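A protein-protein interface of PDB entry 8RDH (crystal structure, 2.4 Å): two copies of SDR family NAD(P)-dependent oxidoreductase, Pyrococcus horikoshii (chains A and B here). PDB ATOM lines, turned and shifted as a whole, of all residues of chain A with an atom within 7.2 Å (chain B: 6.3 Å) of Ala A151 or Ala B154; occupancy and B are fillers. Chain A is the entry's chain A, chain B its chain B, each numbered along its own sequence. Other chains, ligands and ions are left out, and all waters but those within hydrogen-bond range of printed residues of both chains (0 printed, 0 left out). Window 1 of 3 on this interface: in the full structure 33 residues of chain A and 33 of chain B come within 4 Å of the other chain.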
ATOM      1  N   TYR A  93      21.291  -1.978  -7.475  1.00  0.00           N
ATOM      2  CA  TYR A  93      21.160  -0.531  -7.559  1.00  0.00           C
ATOM      3  C   TYR A  93      22.357   0.149  -6.922  1.00  0.00           C
ATOM      4  O   TYR A  93      22.865   1.149  -7.439  1.00  0.00           O
ATOM      5  CB  TYR A  93      19.869  -0.068  -6.886  1.00  0.00           C
ATOM      6  CG  TYR A  93      19.781   1.431  -6.745  1.00  0.00           C
ATOM      7  CD1 TYR A  93      19.356   2.225  -7.801  1.00  0.00           C
ATOM      8  CD2 TYR A  93      20.122   2.054  -5.553  1.00  0.00           C
ATOM      9  CE1 TYR A  93      19.275   3.593  -7.673  1.00  0.00           C
ATOM     10  CE2 TYR A  93      20.044   3.421  -5.417  1.00  0.00           C
ATOM     11  CZ  TYR A  93      19.622   4.184  -6.482  1.00  0.00           C
ATOM     12  OH  TYR A  93      19.531   5.547  -6.356  1.00  0.00           O
ATOM     13  N   ASN A  96      25.746  -0.378  -9.120  1.00  0.00           N
ATOM     14  CA  ASN A  96      25.744   0.000 -10.526  1.00  0.00           C
ATOM     15  C   ASN A  96      25.274   1.426 -10.754  1.00  0.00           C
ATOM     16  O   ASN A  96      25.818   2.109 -11.625  1.00  0.00           O
ATOM     17  CB  ASN A  96      24.867  -0.973 -11.318  1.00  0.00           C
ATOM     18  CG  ASN A  96      25.518  -2.326 -11.496  1.00  0.00           C
ATOM     19  OD1 ASN A  96      26.388  -2.504 -12.349  1.00  0.00           O
ATOM     20  ND2 ASN A  96      25.103  -3.291 -10.684  1.00  0.00           N
ATOM     21  N   VAL A  97      24.281   1.892 -10.007  1.00  0.00           N
ATOM     22  CA  VAL A  97      23.800   3.265 -10.118  1.00  0.00           C
ATOM     23  C   VAL A  97      24.436   4.161  -9.070  1.00  0.00           C
ATOM     24  O   VAL A  97      25.000   5.206  -9.394  1.00  0.00           O
ATOM     25  CB  VAL A  97      22.260   3.310 -10.021  1.00  0.00           C
ATOM     26  CG1 VAL A  97      21.745   4.711 -10.339  1.00  0.00           C
ATOM     27  CG2 VAL A  97      21.643   2.286 -10.951  1.00  0.00           C
ATOM     28  N   THR A 100      28.220   4.704  -9.301  1.00  0.00           N
ATOM     29  CA  THR A 100      28.473   5.492 -10.504  1.00  0.00           C
ATOM     30  C   THR A 100      28.135   6.961 -10.278  1.00  0.00           C
ATOM     31  O   THR A 100      28.889   7.852 -10.684  1.00  0.00           O
ATOM     32  CB  THR A 100      27.673   4.931 -11.679  1.00  0.00           C
ATOM     33  OG1 THR A 100      28.113   3.597 -11.965  1.00  0.00           O
ATOM     34  CG2 THR A 100      27.860   5.796 -12.911  1.00  0.00           C
ATOM     35  N   LEU A 104      30.691  10.103 -10.416  1.00  0.00           N
ATOM     36  CA  LEU A 104      30.485  11.254 -11.289  1.00  0.00           C
ATOM     37  C   LEU A 104      30.547  12.555 -10.503  1.00  0.00           C
ATOM     38  O   LEU A 104      31.101  13.551 -10.982  1.00  0.00           O
ATOM     39  CB  LEU A 104      29.147  11.136 -12.018  1.00  0.00           C
ATOM     40  CG  LEU A 104      29.080  10.047 -13.091  1.00  0.00           C
ATOM     41  CD1 LEU A 104      27.637   9.779 -13.517  1.00  0.00           C
ATOM     42  CD2 LEU A 104      29.939  10.429 -14.294  1.00  0.00           C
ATOM     43  N   PHE A 117      33.492   3.376 -19.402  1.00  0.00           N
ATOM     44  CA  PHE A 117      32.502   2.644 -18.622  1.00  0.00           C
ATOM     45  C   PHE A 117      32.119   1.355 -19.329  1.00  0.00           C
ATOM     46  O   PHE A 117      31.697   1.375 -20.490  1.00  0.00           O
ATOM     47  CB  PHE A 117      31.261   3.512 -18.382  1.00  0.00           C
ATOM     48  CG  PHE A 117      30.160   2.810 -17.646  1.00  0.00           C
ATOM     49  CD1 PHE A 117      30.389   2.249 -16.402  1.00  0.00           C
ATOM     50  CD2 PHE A 117      28.889   2.729 -18.189  1.00  0.00           C
ATOM     51  CE1 PHE A 117      29.373   1.607 -15.719  1.00  0.00           C
ATOM     52  CE2 PHE A 117      27.870   2.090 -17.510  1.00  0.00           C
ATOM     53  CZ  PHE A 117      28.113   1.528 -16.275  1.00  0.00           C
ATOM     54  N   VAL A 123      21.283  -3.841 -21.584  1.00  0.00           N
ATOM     55  CA  VAL A 123      20.541  -2.592 -21.727  1.00  0.00           C
ATOM     56  C   VAL A 123      19.601  -2.653 -22.922  1.00  0.00           C
ATOM     57  O   VAL A 123      18.605  -1.920 -22.963  1.00  0.00           O
ATOM     58  CB  VAL A 123      21.486  -1.381 -21.859  1.00  0.00           C
ATOM     59  CG1 VAL A 123      22.454  -1.321 -20.681  1.00  0.00           C
ATOM     60  CG2 VAL A 123      22.239  -1.416 -23.188  1.00  0.00           C
ATOM     61  N   LEU A 139      15.171   1.281 -25.650  1.00  0.00           N
ATOM     62  CA  LEU A 139      15.918   0.428 -24.733  1.00  0.00           C
ATOM     63  C   LEU A 139      15.010   0.006 -23.583  1.00  0.00           C
ATOM     64  O   LEU A 139      14.511   0.851 -22.833  1.00  0.00           O
ATOM     65  CB  LEU A 139      17.153   1.169 -24.231  1.00  0.00           C
ATOM     66  CG  LEU A 139      18.206   1.312 -25.332  1.00  0.00           C
ATOM     67  CD1 LEU A 139      19.056   2.553 -25.153  1.00  0.00           C
ATOM     68  CD2 LEU A 139      19.083   0.068 -25.367  1.00  0.00           C
ATOM     69  N   GLU A 140      14.804  -1.302 -23.445  1.00  0.00           N
ATOM     70  CA  GLU A 140      13.811  -1.864 -22.530  1.00  0.00           C
ATOM     71  C   GLU A 140      14.443  -3.012 -21.752  1.00  0.00           C
ATOM     72  O   GLU A 140      14.097  -4.183 -21.948  1.00  0.00           O
ATOM     73  CB  GLU A 140      12.578  -2.328 -23.307  1.00  0.00           C
ATOM     74  CG  GLU A 140      11.415  -2.813 -22.453  1.00  0.00           C
ATOM     75  CD  GLU A 140      10.228  -3.254 -23.295  1.00  0.00           C
ATOM     76  OE1 GLU A 140      10.120  -2.800 -24.454  1.00  0.00           O
ATOM     77  OE2 GLU A 140       9.408  -4.056 -22.802  1.00  0.00           O
ATOM     78  N   PRO A 141      15.386  -2.708 -20.860  1.00  0.00           N
ATOM     79  CA  PRO A 141      16.021  -3.771 -20.073  1.00  0.00           C
ATOM     80  C   PRO A 141      14.997  -4.588 -19.302  1.00  0.00           C
ATOM     81  O   PRO A 141      14.023  -4.057 -18.763  1.00  0.00           O
ATOM     82  CB  PRO A 141      16.961  -3.010 -19.130  1.00  0.00           C
ATOM     83  CG  PRO A 141      16.536  -1.575 -19.202  1.00  0.00           C
ATOM     84  CD  PRO A 141      15.949  -1.383 -20.556  1.00  0.00           C
ATOM     85  N   ILE A 142      15.240  -5.899 -19.243  1.00  0.00           N
ATOM     86  CA  ILE A 142      14.342  -6.827 -18.573  1.00  0.00           C
ATOM     87  C   ILE A 142      14.869  -7.269 -17.221  1.00  0.00           C
ATOM     88  O   ILE A 142      14.186  -8.028 -16.520  1.00  0.00           O
ATOM     89  CB  ILE A 142      14.054  -8.051 -19.466  1.00  0.00           C
ATOM     90  CG1 ILE A 142      15.316  -8.903 -19.649  1.00  0.00           C
ATOM     91  CG2 ILE A 142      13.504  -7.606 -20.817  1.00  0.00           C
ATOM     92  CD1 ILE A 142      15.065 -10.219 -20.353  1.00  0.00           C
ATOM     93  N   SER A 143      16.058  -6.820 -16.829  1.00  0.00           N
ATOM     94  CA  SER A 143      16.648  -7.173 -15.549  1.00  0.00           C
ATOM     95  C   SER A 143      16.932  -5.907 -14.755  1.00  0.00           C
ATOM     96  O   SER A 143      17.105  -4.825 -15.323  1.00  0.00           O
ATOM     97  CB  SER A 143      17.948  -7.973 -15.730  1.00  0.00           C
ATOM     98  OG  SER A 143      18.944  -7.198 -16.378  1.00  0.00           O
ATOM     99  N   VAL A 144      16.967  -6.047 -13.430  1.00  0.00           N
ATOM    100  CA  VAL A 144      17.401  -4.937 -12.590  1.00  0.00           C
ATOM    101  C   VAL A 144      18.839  -4.569 -12.923  1.00  0.00           C
ATOM    102  O   VAL A 144      19.214  -3.391 -12.922  1.00  0.00           O
ATOM    103  CB  VAL A 144      17.235  -5.292 -11.101  1.00  0.00           C
ATOM    104  CG1 VAL A 144      17.839  -4.214 -10.227  1.00  0.00           C
ATOM    105  CG2 VAL A 144      15.765  -5.486 -10.768  1.00  0.00           C
ATOM    106  N   TYR A 145      19.660  -5.568 -13.230  1.00  0.00           N
ATOM    107  CA  TYR A 145      21.049  -5.310 -13.592  1.00  0.00           C
ATOM    108  C   TYR A 145      21.151  -4.484 -14.871  1.00  0.00           C
ATOM    109  O   TYR A 145      21.888  -3.491 -14.929  1.00  0.00           O
ATOM    110  CB  TYR A 145      21.780  -6.634 -13.760  1.00  0.00           C
ATOM    111  CG  TYR A 145      23.131  -6.475 -14.381  1.00  0.00           C
ATOM    112  CD1 TYR A 145      24.252  -6.223 -13.608  1.00  0.00           C
ATOM    113  CD2 TYR A 145      23.279  -6.538 -15.753  1.00  0.00           C
ATOM    114  CE1 TYR A 145      25.485  -6.069 -14.187  1.00  0.00           C
ATOM    115  CE2 TYR A 145      24.490  -6.372 -16.336  1.00  0.00           C
ATOM    116  CZ  TYR A 145      25.602  -6.147 -15.556  1.00  0.00           C
ATOM    117  OH  TYR A 145      26.828  -5.997 -16.160  1.00  0.00           O
ATOM    118  N   GLY A 146      20.447  -4.903 -15.923  1.00  0.00           N
ATOM    119  CA  GLY A 146      20.497  -4.154 -17.166  1.00  0.00           C
ATOM    120  C   GLY A 146      19.939  -2.754 -17.011  1.00  0.00           C
ATOM    121  O   GLY A 146      20.499  -1.786 -17.536  1.00  0.00           O
ATOM    122  N   ALA A 147      18.830  -2.627 -16.280  1.00  0.00           N
ATOM    123  CA  ALA A 147      18.286  -1.308 -15.987  1.00  0.00           C
ATOM    124  C   ALA A 147      19.315  -0.438 -15.280  1.00  0.00           C
ATOM    125  O   ALA A 147      19.464   0.747 -15.602  1.00  0.00           O
ATOM    126  CB  ALA A 147      17.027  -1.441 -15.132  1.00  0.00           C
ATOM    127  N   ALA A 148      20.033  -1.009 -14.310  1.00  0.00           N
ATOM    128  CA  ALA A 148      21.027  -0.232 -13.580  1.00  0.00           C
ATOM    129  C   ALA A 148      22.156   0.207 -14.499  1.00  0.00           C
ATOM    130  O   ALA A 148      22.621   1.351 -14.422  1.00  0.00           O
ATOM    131  CB  ALA A 148      21.580  -1.049 -12.414  1.00  0.00           C
ATOM    132  N   LYS A 149      22.606  -0.689 -15.378  1.00  0.00           N
ATOM    133  CA  LYS A 149      23.646  -0.319 -16.332  1.00  0.00           C
ATOM    134  C   LYS A 149      23.183   0.826 -17.229  1.00  0.00           C
ATOM    135  O   LYS A 149      23.947   1.765 -17.502  1.00  0.00           O
ATOM    136  CB  LYS A 149      24.043  -1.538 -17.165  1.00  0.00           C
ATOM    137  CG  LYS A 149      24.923  -2.528 -16.414  1.00  0.00           C
ATOM    138  CD  LYS A 149      26.194  -1.846 -15.950  1.00  0.00           C
ATOM    139  CE  LYS A 149      27.312  -2.815 -15.652  1.00  0.00           C
ATOM    140  NZ  LYS A 149      28.534  -2.058 -15.260  1.00  0.00           N
ATOM    141  N   LEU A 150      21.927   0.780 -17.676  1.00  0.00           N
ATOM    142  CA  LEU A 150      21.419   1.847 -18.535  1.00  0.00           C
ATOM    143  C   LEU A 150      21.319   3.168 -17.780  1.00  0.00           C
ATOM    144  O   LEU A 150      21.643   4.234 -18.326  1.00  0.00           O
ATOM    145  CB  LEU A 150      20.058   1.453 -19.107  1.00  0.00           C
ATOM    146  CG  LEU A 150      19.469   2.457 -20.096  1.00  0.00           C
ATOM    147  CD1 LEU A 150      20.492   2.821 -21.163  1.00  0.00           C
ATOM    148  CD2 LEU A 150      18.211   1.901 -20.727  1.00  0.00           C
ATOM    149  N   ALA A 151      20.856   3.121 -16.532  1.00  0.00           N
ATOM    150  CA  ALA A 151      20.813   4.324 -15.711  1.00  0.00           C
ATOM    151  C   ALA A 151      22.203   4.926 -15.552  1.00  0.00           C
ATOM    152  O   ALA A 151      22.386   6.145 -15.666  1.00  0.00           O
ATOM    153  CB  ALA A 151      20.206   3.998 -14.346  1.00  0.00           C
ATOM    154  N   ALA A 152      23.197   4.081 -15.264  1.00  0.00           N
ATOM    155  CA  ALA A 152      24.570   4.561 -15.141  1.00  0.00           C
ATOM    156  C   ALA A 152      25.024   5.244 -16.425  1.00  0.00           C
ATOM    157  O   ALA A 152      25.603   6.335 -16.385  1.00  0.00           O
ATOM    158  CB  ALA A 152      25.497   3.400 -14.780  1.00  0.00           C
ATOM    159  N   GLU A 153      24.792   4.605 -17.577  1.00  0.00           N
ATOM    160  CA  GLU A 153      25.122   5.236 -18.853  1.00  0.00           C
ATOM    161  C   GLU A 153      24.509   6.630 -18.955  1.00  0.00           C
ATOM    162  O   GLU A 153      25.176   7.597 -19.348  1.00  0.00           O
ATOM    163  CB  GLU A 153      24.622   4.383 -20.020  1.00  0.00           C
ATOM    164  CG  GLU A 153      25.362   3.083 -20.279  1.00  0.00           C
ATOM    165  CD  GLU A 153      24.908   2.431 -21.583  1.00  0.00           C
ATOM    166  OE1 GLU A 153      24.014   2.994 -22.249  1.00  0.00           O
ATOM    167  OE2 GLU A 153      25.450   1.371 -21.957  1.00  0.00           O
ATOM    168  N   ALA A 154      23.213   6.733 -18.646  1.00  0.00           N
ATOM    169  CA  ALA A 154      22.510   8.003 -18.796  1.00  0.00           C
ATOM    170  C   ALA A 154      23.126   9.077 -17.908  1.00  0.00           C
ATOM    171  O   ALA A 154      23.369  10.212 -18.349  1.00  0.00           O
ATOM    172  CB  ALA A 154      21.029   7.815 -18.468  1.00  0.00           C
ATOM    173  N   LEU A 155      23.342   8.746 -16.634  1.00  0.00           N
ATOM    174  CA  LEU A 155      24.005   9.680 -15.730  1.00  0.00           C
ATOM    175  C   LEU A 155      25.365  10.088 -16.273  1.00  0.00           C
ATOM    176  O   LEU A 155      25.740  11.267 -16.214  1.00  0.00           O
ATOM    177  CB  LEU A 155      24.149   9.059 -14.343  1.00  0.00           C
ATOM    178  CG  LEU A 155      22.848   8.766 -13.596  1.00  0.00           C
ATOM    179  CD1 LEU A 155      23.161   8.226 -12.218  1.00  0.00           C
ATOM    180  CD2 LEU A 155      21.981  10.008 -13.501  1.00  0.00           C
ATOM    181  N   ILE A 156      26.135   9.124 -16.780  1.00  0.00           N
ATOM    182  CA  ILE A 156      27.458   9.453 -17.295  1.00  0.00           C
ATOM    183  C   ILE A 156      27.340  10.483 -18.405  1.00  0.00           C
ATOM    184  O   ILE A 156      28.096  11.457 -18.446  1.00  0.00           O
ATOM    185  CB  ILE A 156      28.187   8.187 -17.782  1.00  0.00           C
ATOM    186  CG1 ILE A 156      28.664   7.360 -16.590  1.00  0.00           C
ATOM    187  CG2 ILE A 156      29.366   8.570 -18.675  1.00  0.00           C
ATOM    188  CD1 ILE A 156      29.076   5.964 -16.959  1.00  0.00           C
ATOM    189  N   SER A 157      26.374  10.298 -19.306  1.00  0.00           N
ATOM    190  CA  SER A 157      26.227  11.224 -20.428  1.00  0.00           C
ATOM    191  C   SER A 157      25.837  12.617 -19.944  1.00  0.00           C
ATOM    192  O   SER A 157      26.408  13.628 -20.386  1.00  0.00           O
ATOM    193  CB  SER A 157      25.191  10.688 -21.419  1.00  0.00           C
ATOM    194  OG  SER A 157      24.897  11.648 -22.418  1.00  0.00           O
ATOM    195  N   VAL B  97      15.958  10.039  -9.662  1.00  0.00           N
ATOM    196  CA  VAL B  97      16.436   8.663  -9.631  1.00  0.00           C
ATOM    197  C   VAL B  97      16.099   8.003  -8.303  1.00  0.00           C
ATOM    198  O   VAL B  97      15.500   6.928  -8.263  1.00  0.00           O
ATOM    199  CB  VAL B  97      17.958   8.623  -9.902  1.00  0.00           C
ATOM    200  CG1 VAL B  97      18.427   7.193 -10.140  1.00  0.00           C
ATOM    201  CG2 VAL B  97      18.327   9.524 -11.072  1.00  0.00           C
ATOM    202  N   ALA B 147      19.395  13.129 -17.969  1.00  0.00           N
ATOM    203  CA  ALA B 147      20.036  11.882 -17.570  1.00  0.00           C
ATOM    204  C   ALA B 147      19.264  11.201 -16.448  1.00  0.00           C
ATOM    205  O   ALA B 147      19.080   9.978 -16.462  1.00  0.00           O
ATOM    206  CB  ALA B 147      21.475  12.160 -17.138  1.00  0.00           C
ATOM    207  N   LYS B 149      16.054  11.526 -15.709  1.00  0.00           N
ATOM    208  CA  LYS B 149      14.805  11.007 -16.262  1.00  0.00           C
ATOM    209  C   LYS B 149      15.033   9.695 -17.004  1.00  0.00           C
ATOM    210  O   LYS B 149      14.242   8.747 -16.876  1.00  0.00           O
ATOM    211  CB  LYS B 149      14.173  12.049 -17.186  1.00  0.00           C
ATOM    212  CG  LYS B 149      13.459  13.172 -16.456  1.00  0.00           C
ATOM    213  CD  LYS B 149      12.355  12.585 -15.609  1.00  0.00           C
ATOM    214  CE  LYS B 149      11.285  13.583 -15.268  1.00  0.00           C
ATOM    215  NZ  LYS B 149      10.214  12.900 -14.503  1.00  0.00           N
ATOM    216  N   LEU B 150      16.117   9.615 -17.775  1.00  0.00           N
ATOM    217  CA  LEU B 150      16.397   8.380 -18.497  1.00  0.00           C
ATOM    218  C   LEU B 150      16.712   7.243 -17.529  1.00  0.00           C
ATOM    219  O   LEU B 150      16.262   6.104 -17.722  1.00  0.00           O
ATOM    220  CB  LEU B 150      17.548   8.612 -19.475  1.00  0.00           C
ATOM    221  CG  LEU B 150      17.913   7.467 -20.415  1.00  0.00           C
ATOM    222  CD1 LEU B 150      16.681   6.951 -21.122  1.00  0.00           C
ATOM    223  CD2 LEU B 150      18.959   7.930 -21.419  1.00  0.00           C
ATOM    224  N   ALA B 151      17.480   7.540 -16.474  1.00  0.00           N
ATOM    225  CA  ALA B 151      17.768   6.544 -15.444  1.00  0.00           C
ATOM    226  C   ALA B 151      16.486   6.017 -14.813  1.00  0.00           C
ATOM    227  O   ALA B 151      16.343   4.809 -14.566  1.00  0.00           O
ATOM    228  CB  ALA B 151      18.673   7.155 -14.372  1.00  0.00           C
ATOM    229  N   ALA B 152      15.562   6.924 -14.497  1.00  0.00           N
ATOM    230  CA  ALA B 152      14.274   6.514 -13.952  1.00  0.00           C
ATOM    231  C   ALA B 152      13.554   5.568 -14.907  1.00  0.00           C
ATOM    232  O   ALA B 152      13.039   4.522 -14.492  1.00  0.00           O
ATOM    233  CB  ALA B 152      13.423   7.748 -13.664  1.00  0.00           C
ATOM    234  N   GLU B 153      13.488   5.936 -16.193  1.00  0.00           N
ATOM    235  CA  GLU B 153      12.876   5.056 -17.190  1.00  0.00           C
ATOM    236  C   GLU B 153      13.483   3.661 -17.139  1.00  0.00           C
ATOM    237  O   GLU B 153      12.769   2.646 -17.148  1.00  0.00           O
ATOM    238  CB  GLU B 153      13.051   5.625 -18.602  1.00  0.00           C
ATOM    239  CG  GLU B 153      12.231   6.861 -18.941  1.00  0.00           C
ATOM    240  CD  GLU B 153      12.305   7.219 -20.425  1.00  0.00           C
ATOM    241  OE1 GLU B 153      12.990   6.503 -21.185  1.00  0.00           O
ATOM    242  OE2 GLU B 153      11.678   8.216 -20.837  1.00  0.00           O
ATOM    243  N   ALA B 154      14.814   3.596 -17.135  1.00  0.00           N
ATOM    244  CA  ALA B 154      15.486   2.303 -17.182  1.00  0.00           C
ATOM    245  C   ALA B 154      15.122   1.458 -15.968  1.00  0.00           C
ATOM    246  O   ALA B 154      14.759   0.280 -16.099  1.00  0.00           O
ATOM    247  CB  ALA B 154      16.998   2.505 -17.269  1.00  0.00           C
ATOM    248  N   LEU B 155      15.227   2.045 -14.772  1.00  0.00           N
ATOM    249  CA  LEU B 155      14.840   1.308 -13.573  1.00  0.00           C
ATOM    250  C   LEU B 155      13.403   0.813 -13.670  1.00  0.00           C
ATOM    251  O   LEU B 155      13.103  -0.330 -13.299  1.00  0.00           O
ATOM    252  CB  LEU B 155      15.008   2.172 -12.325  1.00  0.00           C
ATOM    253  CG  LEU B 155      16.422   2.600 -11.940  1.00  0.00           C
ATOM    254  CD1 LEU B 155      16.360   3.355 -10.621  1.00  0.00           C
ATOM    255  CD2 LEU B 155      17.354   1.408 -11.846  1.00  0.00           C
ATOM    256  N   ILE B 156      12.489   1.671 -14.134  1.00  0.00           N
ATOM    257  CA  ILE B 156      11.091   1.263 -14.224  1.00  0.00           C
ATOM    258  C   ILE B 156      10.955   0.046 -15.125  1.00  0.00           C
ATOM    259  O   ILE B 156      10.219  -0.897 -14.810  1.00  0.00           O
ATOM    260  CB  ILE B 156      10.216   2.430 -14.715  1.00  0.00           C
ATOM    261  CG1 ILE B 156      10.038   3.455 -13.595  1.00  0.00           C
ATOM    262  CG2 ILE B 156       8.866   1.907 -15.189  1.00  0.00           C
ATOM    263  CD1 ILE B 156       9.504   4.789 -14.072  1.00  0.00           C
ATOM    264  N   SER B 157      11.670   0.039 -16.251  1.00  0.00           N
ATOM    265  CA  SER B 157      11.567  -1.084 -17.179  1.00  0.00           C
ATOM    266  C   SER B 157      12.083  -2.367 -16.541  1.00  0.00           C
ATOM    267  O   SER B 157      11.420  -3.419 -16.584  1.00  0.00           O
ATOM    268  CB  SER B 157      12.347  -0.771 -18.458  1.00  0.00           C
ATOM    269  OG  SER B 157      12.433  -1.903 -19.305  1.00  0.00           O
ATOM    270  N   GLY B 158      13.268  -2.295 -15.935  1.00  0.00           N
ATOM    271  CA  GLY B 158      13.834  -3.480 -15.319  1.00  0.00           C
ATOM    272  C   GLY B 158      12.942  -4.042 -14.232  1.00  0.00           C
ATOM    273  O   GLY B 158      12.725  -5.255 -14.158  1.00  0.00           O
ATOM    274  N   TYR B 159      12.391  -3.167 -13.386  1.00  0.00           N
ATOM    275  CA  TYR B 159      11.521  -3.640 -12.315  1.00  0.00           C
ATOM    276  C   TYR B 159      10.226  -4.216 -12.874  1.00  0.00           C
ATOM    277  O   TYR B 159       9.745  -5.246 -12.393  1.00  0.00           O
ATOM    278  CB  TYR B 159      11.221  -2.507 -11.338  1.00  0.00           C
ATOM    279  CG  TYR B 159      12.219  -2.394 -10.213  1.00  0.00           C
ATOM    280  CD1 TYR B 159      13.479  -1.862 -10.436  1.00  0.00           C
ATOM    281  CD2 TYR B 159      11.908  -2.826  -8.931  1.00  0.00           C
ATOM    282  CE1 TYR B 159      14.398  -1.753  -9.418  1.00  0.00           C
ATOM    283  CE2 TYR B 159      12.821  -2.719  -7.900  1.00  0.00           C
ATOM    284  CZ  TYR B 159      14.067  -2.182  -8.152  1.00  0.00           C
ATOM    285  OH  TYR B 159      14.993  -2.069  -7.139  1.00  0.00           O
ATOM    286  N   ILE B 169       5.621   4.573 -20.126  1.00  0.00           N
ATOM    287  CA  ILE B 169       6.553   5.693 -20.056  1.00  0.00           C
ATOM    288  C   ILE B 169       6.128   6.716 -21.101  1.00  0.00           C
ATOM    289  O   ILE B 169       6.060   6.397 -22.294  1.00  0.00           O
ATOM    290  CB  ILE B 169       7.999   5.221 -20.281  1.00  0.00           C
ATOM    291  CG1 ILE B 169       8.472   4.399 -19.081  1.00  0.00           C
ATOM    292  CG2 ILE B 169       8.928   6.397 -20.534  1.00  0.00           C
ATOM    293  CD1 ILE B 169       9.544   3.389 -19.419  1.00  0.00           C
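The backbone carbonyl oxygen (O) of Pro A141 is in hydrogen-bond range of the side-chain hydroxyl (OG) of Ser B157.
O of Pro A141 lies within hydrogen-bond range of N of Gly B158 (3.4 Å).
N of Gly A146 lies within hydrogen-bond range of OG of Ser A143 (2.8 Å).
Ala A147 touches Ala B154, and with the chains exchanged Ala A154 touches Ala B147.
Ala A147 touches Leu B155, and with the chains exchanged Leu A155 touches Ala B147.
Leu A150 touches Ala B154, and with the chains exchanged Ala A154 touches Leu B150.
Ala A151 touches Ala B154, but with the chains exchanged Ala A154 does not touch Ala B151 (4.1 Å).
11 positions are printed for both chains.
Ala A151 touches just these residues of chain B: Ala B151 and Ala B154.
Ala B154 touches just these residues of chain A: Ala A147 (3.0 Å), Leu A150 (3.7 Å) and Ala A151 (3.98 Å).
Of the printed residues of chain B, Leu A150 touches Ala B154 (3.7 Å).
Printed residues of chain A within 4 Å of Leu B155: Ala A147 (3.8 Å).
Printed residues of chain B within 4 Å of Ile A142: Gly B158 (3.9 Å).
The nearest residue of chain B that does not touch Ala A151 is Leu B155 (4.6 Å).
The nearest residue of chain A that does not touch Ala B154 is Pro A141 (4.03 Å).
The nearest printed residue of chain B that does not touch Ser A143 is Tyr B159 (5.4 Å).
Printed residues of chain B that touch a printed residue of chain A: Ala B147, Leu B150, Ala B151, Ala B154, Leu B155, Ser B157 and Gly B158.
Hydrophobic or aromatic side chains of chain B within 4 Å of the printed part of chain A: Ala B147, Leu B150, Ala B151 and Ala B154.
Of the 26 printed residues of chain A, 9 touch a printed residue of chain B.
Printed residues of chain A that touch a printed residue of chain B: Glu A140, Pro A141, Ile A142, Ser A143, Ala A147, Leu A150, Ala A151, Ala A154 and Leu A155.
Hydrophobic or aromatic side chains of chain A within 4 Å of the printed part of chain B: Pro A141, Ala A147, Leu A150, Ala A151 and Ala A154.
Among the printed residues, no Asp or Glu carboxylate lies within 4 Å of a Lys or Arg side-chain nitrogen of the other chain.
Among the printed residues, pairs that only touch across the chains: Ala A154 with Ala B147 (3.0 Å), Ala A147 with Ala B154 (3.0 Å), Glu A140 with Ser B157 (3.4 Å), Ala A151 with Ala B151 (3.5 Å), Ser A143 with Gly B158 (3.5 Å), Ala A154 with Leu B150 (3.6 Å), Leu A150 with Ala B154 (3.7 Å), Ala A147 with Gly B158 (3.8 Å), Leu A155 with Ala B147 (3.8 Å), Ala A147 with Leu B155 (3.8 Å), Ile A142 with Gly B158 (3.9 Å) and Ala A151 with Ala B154 (3.98 Å).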
